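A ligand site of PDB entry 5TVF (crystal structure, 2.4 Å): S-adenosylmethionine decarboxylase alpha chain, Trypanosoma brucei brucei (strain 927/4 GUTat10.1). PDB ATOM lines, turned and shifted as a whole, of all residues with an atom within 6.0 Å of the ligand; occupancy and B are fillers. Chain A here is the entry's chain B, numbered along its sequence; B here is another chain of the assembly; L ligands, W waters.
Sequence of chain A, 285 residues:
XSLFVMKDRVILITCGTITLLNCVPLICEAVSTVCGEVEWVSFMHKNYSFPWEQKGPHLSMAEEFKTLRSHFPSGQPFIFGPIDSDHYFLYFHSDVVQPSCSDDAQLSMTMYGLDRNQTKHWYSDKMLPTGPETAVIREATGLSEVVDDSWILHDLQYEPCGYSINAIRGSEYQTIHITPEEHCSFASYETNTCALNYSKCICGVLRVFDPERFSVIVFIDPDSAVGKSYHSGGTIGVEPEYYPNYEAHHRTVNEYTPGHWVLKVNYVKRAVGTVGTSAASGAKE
An oxygen (O2) of the ligand sits at hydrogen-bond distance from the side-chain hydroxyl of Ser 102, 2.5 Å away.
The guanidinium group of Arg 9 sits at hydrogen-bond distance from an oxygen (O5) of the ligand (2.5 Å).
OE2 of Glu 36 of chain B is in hydrogen-bond range of O5 of the ligand.
A nitrogen (N1) of the ligand is in salt-bridge range of the side-chain carboxylate (OD2) of Asp 221 (3.1 Å).
O6 of the ligand sits at hydrogen-bond distance from OH of Tyr 256, 3.4 Å away.
An oxygen (O2) of the ligand lies within hydrogen-bond range of the backbone carbonyl oxygen (O) of Cys 101 (3.5 Å).
A nitrogen (N1) of the ligand is in salt-bridge range of the side-chain carboxylate (OD2) of Asp 104, 3.6 Å away.
The guanidinium group of Arg 9 is in salt-bridge range of the side-chain carboxylate of Glu 36 of chain B (3.1 Å).
NH1 of Arg 9 is in salt-bridge range of OD2 of Asp 104, at 2.6 Å.
The side-chain carboxylate (OE1) of Glu 36 of chain B lies within salt-bridge range of the guanidinium group (NH1) of Arg 34 of chain B, at 2.8 Å.
The side-chain carboxylate (OD2) of Asp 221 sits at hydrogen-bond distance from the backbone NH (N) of Asp 104, at 2.9 Å.
O of Trp 40 sits at hydrogen-bond distance from N of Ile 38 of chain B (2.9 Å).
The backbone NH (N) of Glu 39 lies within hydrogen-bond range of the backbone carbonyl oxygen (O) of Ile 38 of chain B, at 3.0 Å.
O of Gln 106 is in hydrogen-bond range of N of Phe 219, at 3.2 Å.
The side-chain amide nitrogen (NE2) of Gln 106 sits close to the guanidinium group (NE) of Arg 34 of chain B (3.3 Å).
Merely in contact with the ligand: Glu 39 (3.3 Å), Trp 40 (3.2 Å), Val 96 (3.6 Å), Ser 100 (3.7 Å), Ala 105 (3.6 Å), Gln 106 (3.9 Å), Phe 219 (3.4 Å), His 260 (3.8 Å) and Ile 38 of chain B (3.5 Å).
Hydrophobic or aromatic side chains that line the ligand: Trp 40, Val 96, Phe 219 and Ile 38 of chain B.
Of the 22 residues printed, 16 come within 4 Å of the ligand.
The nearest printed residue that does not touch the ligand is Ile 220 (4.8 Å).
Water W2 lies within hydrogen-bond range of the side-chain hydroxyl (OG) of Ser 42 (2.5 Å), the side-chain carboxylate (OE1) of Glu 36 of chain B (2.7 Å) and the indole nitrogen (NE1) of Trp 40 (2.9 Å).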
ATOM      1  N   ARG A   9      34.126  33.277   8.485  1.00  0.00           N
ATOM      2  CA  ARG A   9      34.975  32.122   8.195  1.00  0.00           C
ATOM      3  C   ARG A   9      36.031  32.488   7.153  1.00  0.00           C
ATOM      4  O   ARG A   9      35.992  33.546   6.538  1.00  0.00           O
ATOM      5  CB  ARG A   9      34.143  30.932   7.710  1.00  0.00           C
ATOM      6  CG  ARG A   9      33.570  31.107   6.311  1.00  0.00           C
ATOM      7  CD  ARG A   9      32.591  30.003   5.969  1.00  0.00           C
ATOM      8  NE  ARG A   9      31.438  30.024   6.855  1.00  0.00           N
ATOM      9  CZ  ARG A   9      30.525  29.061   6.921  1.00  0.00           C
ATOM     10  NH1 ARG A   9      29.510  29.182   7.769  1.00  0.00           N
ATOM     11  NH2 ARG A   9      30.620  27.989   6.156  1.00  0.00           N
ATOM     12  N   ILE A  11      38.099  30.228   3.898  1.00  0.00           N
ATOM     13  CA  ILE A  11      38.186  28.999   3.114  1.00  0.00           C
ATOM     14  C   ILE A  11      39.411  29.132   2.224  1.00  0.00           C
ATOM     15  O   ILE A  11      39.409  29.927   1.267  1.00  0.00           O
ATOM     16  CB  ILE A  11      36.920  28.755   2.268  1.00  0.00           C
ATOM     17  CG1 ILE A  11      35.719  28.507   3.190  1.00  0.00           C
ATOM     18  CG2 ILE A  11      37.128  27.580   1.309  1.00  0.00           C
ATOM     19  CD1 ILE A  11      34.389  28.432   2.460  1.00  0.00           C
ATOM     20  N   GLU A  39      35.425  28.024  16.424  1.00  0.00           N
ATOM     21  CA  GLU A  39      34.526  26.953  16.833  1.00  0.00           C
ATOM     22  C   GLU A  39      34.501  25.767  15.899  1.00  0.00           C
ATOM     23  O   GLU A  39      33.927  24.729  16.242  1.00  0.00           O
ATOM     24  CB  GLU A  39      33.089  27.473  16.963  1.00  0.00           C
ATOM     25  CG  GLU A  39      32.525  28.098  15.673  1.00  0.00           C
ATOM     26  CD  GLU A  39      31.010  28.278  15.721  1.00  0.00           C
ATOM     27  OE1 GLU A  39      30.344  27.604  16.530  1.00  0.00           O
ATOM     28  OE2 GLU A  39      30.488  29.102  14.928  1.00  0.00           O
ATOM     29  N   TRP A  40      35.080  25.880  14.704  1.00  0.00           N
ATOM     30  CA  TRP A  40      34.923  24.855  13.687  1.00  0.00           C
ATOM     31  C   TRP A  40      36.101  24.946  12.747  1.00  0.00           C
ATOM     32  O   TRP A  40      36.318  25.989  12.120  1.00  0.00           O
ATOM     33  CB  TRP A  40      33.603  25.055  12.945  1.00  0.00           C
ATOM     34  CG  TRP A  40      33.332  24.054  11.867  1.00  0.00           C
ATOM     35  CD1 TRP A  40      33.940  23.982  10.650  1.00  0.00           C
ATOM     36  CD2 TRP A  40      32.367  22.997  11.898  1.00  0.00           C
ATOM     37  NE1 TRP A  40      33.418  22.935   9.918  1.00  0.00           N
ATOM     38  CE2 TRP A  40      32.454  22.319  10.665  1.00  0.00           C
ATOM     39  CE3 TRP A  40      31.435  22.559  12.848  1.00  0.00           C
ATOM     40  CZ2 TRP A  40      31.644  21.224  10.360  1.00  0.00           C
ATOM     41  CZ3 TRP A  40      30.639  21.482  12.547  1.00  0.00           C
ATOM     42  CH2 TRP A  40      30.747  20.817  11.315  1.00  0.00           C
ATOM     43  N   SER A  42      38.074  22.500   9.693  1.00  0.00           N
ATOM     44  CA  SER A  42      38.111  21.295   8.878  1.00  0.00           C
ATOM     45  C   SER A  42      39.304  21.387   7.938  1.00  0.00           C
ATOM     46  O   SER A  42      39.528  22.434   7.316  1.00  0.00           O
ATOM     47  CB  SER A  42      36.821  21.123   8.074  1.00  0.00           C
ATOM     48  OG  SER A  42      36.721  22.094   7.052  1.00  0.00           O
ATOM     49  N   VAL A  96      31.810  23.793  19.613  1.00  0.00           N
ATOM     50  CA  VAL A  96      30.511  24.456  19.597  1.00  0.00           C
ATOM     51  C   VAL A  96      29.953  24.400  21.021  1.00  0.00           C
ATOM     52  O   VAL A  96      29.428  23.365  21.445  1.00  0.00           O
ATOM     53  CB  VAL A  96      29.545  23.819  18.593  1.00  0.00           C
ATOM     54  CG1 VAL A  96      28.235  24.597  18.529  1.00  0.00           C
ATOM     55  CG2 VAL A  96      30.185  23.746  17.214  1.00  0.00           C
ATOM     56  N   SER A 100      23.602  26.175  17.653  1.00  0.00           N
ATOM     57  CA  SER A 100      23.253  27.176  16.659  1.00  0.00           C
ATOM     58  C   SER A 100      22.454  26.493  15.545  1.00  0.00           C
ATOM     59  O   SER A 100      22.029  25.340  15.679  1.00  0.00           O
ATOM     60  CB  SER A 100      24.523  27.859  16.127  1.00  0.00           C
ATOM     61  OG  SER A 100      25.271  28.429  17.184  1.00  0.00           O
ATOM     62  N   CYS A 101      22.259  27.223  14.451  1.00  0.00           N
ATOM     63  CA  CYS A 101      21.516  26.740  13.295  1.00  0.00           C
ATOM     64  C   CYS A 101      22.481  26.586  12.125  1.00  0.00           C
ATOM     65  O   CYS A 101      23.066  27.572  11.670  1.00  0.00           O
ATOM     66  CB  CYS A 101      20.380  27.706  12.950  1.00  0.00           C
ATOM     67  SG  CYS A 101      19.428  27.268  11.475  1.00  0.00           S
ATOM     68  N   SER A 102      22.635  25.347  11.643  1.00  0.00           N
ATOM     69  CA  SER A 102      23.569  25.039  10.569  1.00  0.00           C
ATOM     70  C   SER A 102      22.781  24.877   9.270  1.00  0.00           C
ATOM     71  O   SER A 102      22.100  23.872   9.071  1.00  0.00           O
ATOM     72  CB  SER A 102      24.348  23.771  10.888  1.00  0.00           C
ATOM     73  OG  SER A 102      25.054  23.893  12.108  1.00  0.00           O
ATOM     74  N   ASP A 103      22.904  25.874   8.384  1.00  0.00           N
ATOM     75  CA  ASP A 103      22.195  25.863   7.110  1.00  0.00           C
ATOM     76  C   ASP A 103      23.137  26.113   5.929  1.00  0.00           C
ATOM     77  O   ASP A 103      22.684  26.548   4.862  1.00  0.00           O
ATOM     78  CB  ASP A 103      21.072  26.899   7.119  1.00  0.00           C
ATOM     79  CG  ASP A 103      21.500  28.230   7.726  1.00  0.00           C
ATOM     80  OD1 ASP A 103      22.565  28.272   8.379  1.00  0.00           O
ATOM     81  OD2 ASP A 103      20.764  29.226   7.548  1.00  0.00           O
ATOM     82  N   ASP A 104      24.426  25.858   6.097  1.00  0.00           N
ATOM     83  CA  ASP A 104      25.384  26.016   5.009  1.00  0.00           C
ATOM     84  C   ASP A 104      25.267  24.860   4.020  1.00  0.00           C
ATOM     85  O   ASP A 104      24.493  23.918   4.202  1.00  0.00           O
ATOM     86  CB  ASP A 104      26.802  26.122   5.554  1.00  0.00           C
ATOM     87  CG  ASP A 104      26.997  27.297   6.468  1.00  0.00           C
ATOM     88  OD1 ASP A 104      26.295  28.324   6.294  1.00  0.00           O
ATOM     89  OD2 ASP A 104      27.865  27.210   7.363  1.00  0.00           O
ATOM     90  N   ALA A 105      26.073  24.925   2.965  1.00  0.00           N
ATOM     91  CA  ALA A 105      26.135  23.881   1.965  1.00  0.00           C
ATOM     92  C   ALA A 105      27.525  23.863   1.360  1.00  0.00           C
ATOM     93  O   ALA A 105      28.187  24.909   1.261  1.00  0.00           O
ATOM     94  CB  ALA A 105      25.075  24.075   0.874  1.00  0.00           C
ATOM     95  N   GLN A 106      27.979  22.679   0.967  1.00  0.00           N
ATOM     96  CA  GLN A 106      29.297  22.523   0.370  1.00  0.00           C
ATOM     97  C   GLN A 106      29.242  21.381  -0.637  1.00  0.00           C
ATOM     98  O   GLN A 106      28.877  20.257  -0.279  1.00  0.00           O
ATOM     99  CB  GLN A 106      30.359  22.254   1.431  1.00  0.00           C
ATOM    100  CG  GLN A 106      31.762  22.073   0.878  1.00  0.00           C
ATOM    101  CD  GLN A 106      32.774  21.824   1.965  1.00  0.00           C
ATOM    102  OE1 GLN A 106      32.513  22.078   3.142  1.00  0.00           O
ATOM    103  NE2 GLN A 106      33.946  21.318   1.592  1.00  0.00           N
ATOM    104  N   PHE A 219      28.610  17.891   1.814  1.00  0.00           N
ATOM    105  CA  PHE A 219      28.419  18.083   3.245  1.00  0.00           C
ATOM    106  C   PHE A 219      27.021  18.636   3.478  1.00  0.00           C
ATOM    107  O   PHE A 219      26.656  19.679   2.933  1.00  0.00           O
ATOM    108  CB  PHE A 219      29.471  19.017   3.820  1.00  0.00           C
ATOM    109  CG  PHE A 219      30.824  18.381   3.962  1.00  0.00           C
ATOM    110  CD1 PHE A 219      31.686  18.295   2.877  1.00  0.00           C
ATOM    111  CD2 PHE A 219      31.229  17.843   5.174  1.00  0.00           C
ATOM    112  CE1 PHE A 219      32.924  17.702   2.997  1.00  0.00           C
ATOM    113  CE2 PHE A 219      32.468  17.243   5.300  1.00  0.00           C
ATOM    114  CZ  PHE A 219      33.315  17.181   4.213  1.00  0.00           C
ATOM    115  N   ILE A 220      26.236  17.921   4.288  1.00  0.00           N
ATOM    116  CA  ILE A 220      24.834  18.243   4.507  1.00  0.00           C
ATOM    117  C   ILE A 220      24.672  18.756   5.935  1.00  0.00           C
ATOM    118  O   ILE A 220      24.990  18.034   6.891  1.00  0.00           O
ATOM    119  CB  ILE A 220      23.936  17.022   4.255  1.00  0.00           C
ATOM    120  CG1 ILE A 220      24.046  16.583   2.793  1.00  0.00           C
ATOM    121  CG2 ILE A 220      22.489  17.329   4.632  1.00  0.00           C
ATOM    122  CD1 ILE A 220      23.264  15.328   2.464  1.00  0.00           C
ATOM    123  N   ASP A 221      24.191  19.980   6.075  1.00  0.00           N
ATOM    124  CA  ASP A 221      23.854  20.498   7.389  1.00  0.00           C
ATOM    125  C   ASP A 221      22.395  20.224   7.717  1.00  0.00           C
ATOM    126  O   ASP A 221      21.556  20.128   6.818  1.00  0.00           O
ATOM    127  CB  ASP A 221      24.121  22.003   7.455  1.00  0.00           C
ATOM    128  CG  ASP A 221      25.582  22.351   7.313  1.00  0.00           C
ATOM    129  OD1 ASP A 221      26.430  21.427   7.401  1.00  0.00           O
ATOM    130  OD2 ASP A 221      25.900  23.534   7.123  1.00  0.00           O
ATOM    131  N   TYR A 256      29.781  12.528  10.557  1.00  0.00           N
ATOM    132  CA  TYR A 256      31.079  12.759  11.195  1.00  0.00           C
ATOM    133  C   TYR A 256      30.932  13.490  12.527  1.00  0.00           C
ATOM    134  O   TYR A 256      31.740  13.275  13.441  1.00  0.00           O
ATOM    135  CB  TYR A 256      31.998  13.523  10.252  1.00  0.00           C
ATOM    136  CG  TYR A 256      31.487  14.864   9.776  1.00  0.00           C
ATOM    137  CD1 TYR A 256      30.686  14.959   8.651  1.00  0.00           C
ATOM    138  CD2 TYR A 256      31.814  16.035  10.445  1.00  0.00           C
ATOM    139  CE1 TYR A 256      30.207  16.180   8.201  1.00  0.00           C
ATOM    140  CE2 TYR A 256      31.356  17.262  10.001  1.00  0.00           C
ATOM    141  CZ  TYR A 256      30.549  17.328   8.889  1.00  0.00           C
ATOM    142  OH  TYR A 256      30.085  18.542   8.446  1.00  0.00           O
ATOM    143  N   HIS A 260      25.323  16.376  11.499  1.00  0.00           N
ATOM    144  CA  HIS A 260      25.944  16.744  10.236  1.00  0.00           C
ATOM    145  C   HIS A 260      26.420  15.504   9.505  1.00  0.00           C
ATOM    146  O   HIS A 260      26.998  14.592  10.109  1.00  0.00           O
ATOM    147  CB  HIS A 260      27.121  17.704  10.458  1.00  0.00           C
ATOM    148  CG  HIS A 260      26.743  18.977  11.147  1.00  0.00           C
ATOM    149  ND1 HIS A 260      26.235  19.000  12.428  1.00  0.00           N
ATOM    150  CD2 HIS A 260      26.792  20.265  10.732  1.00  0.00           C
ATOM    151  CE1 HIS A 260      25.991  20.255  12.773  1.00  0.00           C
ATOM    152  NE2 HIS A 260      26.323  21.038  11.760  1.00  0.00           N
ATOM    153  N   TRP A 261      26.173  15.464   8.196  1.00  0.00           N
ATOM    154  CA  TRP A 261      26.449  14.301   7.376  1.00  0.00           C
ATOM    155  C   TRP A 261      27.287  14.692   6.166  1.00  0.00           C
ATOM    156  O   TRP A 261      27.292  15.851   5.736  1.00  0.00           O
ATOM    157  CB  TRP A 261      25.144  13.642   6.893  1.00  0.00           C
ATOM    158  CG  TRP A 261      24.328  13.072   7.994  1.00  0.00           C
ATOM    159  CD1 TRP A 261      23.587  13.766   8.918  1.00  0.00           C
ATOM    160  CD2 TRP A 261      24.150  11.686   8.309  1.00  0.00           C
ATOM    161  NE1 TRP A 261      22.964  12.895   9.770  1.00  0.00           N
ATOM    162  CE2 TRP A 261      23.294  11.619   9.427  1.00  0.00           C
ATOM    163  CE3 TRP A 261      24.636  10.500   7.755  1.00  0.00           C
ATOM    164  CZ2 TRP A 261      22.914  10.403   9.988  1.00  0.00           C
ATOM    165  CZ3 TRP A 261      24.256   9.300   8.320  1.00  0.00           C
ATOM    166  CH2 TRP A 261      23.405   9.261   9.425  1.00  0.00           C
ATOM    167  N   ARG B  34      42.233  21.770   1.343  1.00  0.00           N
ATOM    168  CA  ARG B  34      41.180  22.702   1.713  1.00  0.00           C
ATOM    169  C   ARG B  34      41.192  22.911   3.222  1.00  0.00           C
ATOM    170  O   ARG B  34      41.147  21.945   3.986  1.00  0.00           O
ATOM    171  CB  ARG B  34      39.805  22.186   1.267  1.00  0.00           C
ATOM    172  CG  ARG B  34      38.674  23.190   1.474  1.00  0.00           C
ATOM    173  CD  ARG B  34      37.330  22.590   1.097  1.00  0.00           C
ATOM    174  NE  ARG B  34      36.258  23.577   1.140  1.00  0.00           N
ATOM    175  CZ  ARG B  34      35.591  23.921   2.233  1.00  0.00           C
ATOM    176  NH1 ARG B  34      35.878  23.355   3.399  1.00  0.00           N
ATOM    177  NH2 ARG B  34      34.630  24.834   2.167  1.00  0.00           N
ATOM    178  N   GLU B  36      39.231  25.230   6.261  1.00  0.00           N
ATOM    179  CA  GLU B  36      38.104  26.086   6.589  1.00  0.00           C
ATOM    180  C   GLU B  36      38.079  26.331   8.094  1.00  0.00           C
ATOM    181  O   GLU B  36      38.152  25.392   8.888  1.00  0.00           O
ATOM    182  CB  GLU B  36      36.775  25.473   6.132  1.00  0.00           C
ATOM    183  CG  GLU B  36      35.583  26.390   6.362  1.00  0.00           C
ATOM    184  CD  GLU B  36      34.303  25.878   5.726  1.00  0.00           C
ATOM    185  OE1 GLU B  36      34.284  24.709   5.288  1.00  0.00           O
ATOM    186  OE2 GLU B  36      33.326  26.647   5.657  1.00  0.00           O
ATOM    187  N   ILE B  38      35.772  28.532  10.921  1.00  0.00           N
ATOM    188  CA  ILE B  38      34.590  29.321  11.247  1.00  0.00           C
ATOM    189  C   ILE B  38      34.714  29.772  12.700  1.00  0.00           C
ATOM    190  O   ILE B  38      35.036  28.963  13.582  1.00  0.00           O
ATOM    191  CB  ILE B  38      33.301  28.517  11.029  1.00  0.00           C
ATOM    192  CG1 ILE B  38      33.253  27.924   9.621  1.00  0.00           C
ATOM    193  CG2 ILE B  38      32.081  29.402  11.284  1.00  0.00           C
ATOM    194  CD1 ILE B  38      32.156  26.906   9.404  1.00  0.00           C
HETATM  195  C1  LIG L   1      28.461  23.997   9.782  1.00  0.00           C
HETATM  196  C2  LIG L   1      28.937  24.775  10.960  1.00  0.00           C
HETATM  197  C3  LIG L   1      29.563  23.885   8.785  1.00  0.00           C
HETATM  198  N1  LIG L   1      28.978  23.820   7.425  1.00  0.00           N
HETATM  199  C4  LIG L   1      29.972  23.395   6.394  1.00  0.00           C
HETATM  200  C5  LIG L   1      29.393  23.548   4.985  1.00  0.00           C
HETATM  201  C6  LIG L   1      31.320  24.185   6.498  1.00  0.00           C
HETATM  202  C7  LIG L   1      30.290  21.843   6.585  1.00  0.00           C
HETATM  203  N2  LIG L   1      27.770  25.183  11.768  1.00  0.00           N
HETATM  204  C8  LIG L   1      28.142  25.658  13.132  1.00  0.00           C
HETATM  205  C9  LIG L   1      28.518  24.503  14.078  1.00  0.00           C
HETATM  206  C10 LIG L   1      26.962  26.454  13.752  1.00  0.00           C
HETATM  207  C11 LIG L   1      29.407  26.665  13.046  1.00  0.00           C
HETATM  208  O1  LIG L   1      27.400  23.710  14.233  1.00  0.00           O
HETATM  209  O2  LIG L   1      25.814  26.017  13.125  1.00  0.00           O
HETATM  210  O3  LIG L   1      30.562  25.907  12.996  1.00  0.00           O
HETATM  211  O4  LIG L   1      28.210  22.859   4.952  1.00  0.00           O
HETATM  212  O5  LIG L   1      31.002  25.518   6.403  1.00  0.00           O
HETATM  213  O6  LIG L   1      29.102  21.151   6.454  1.00  0.00           O
HETATM  214  O   HOH W   1      27.222  21.001  16.044  1.00  0.00           O
HETATM  215  O   HOH W   2      34.365  22.764   7.174  1.00  0.00           O
HETATM  216  O   HOH W   3      27.755  18.716   7.149  1.00  0.00           O
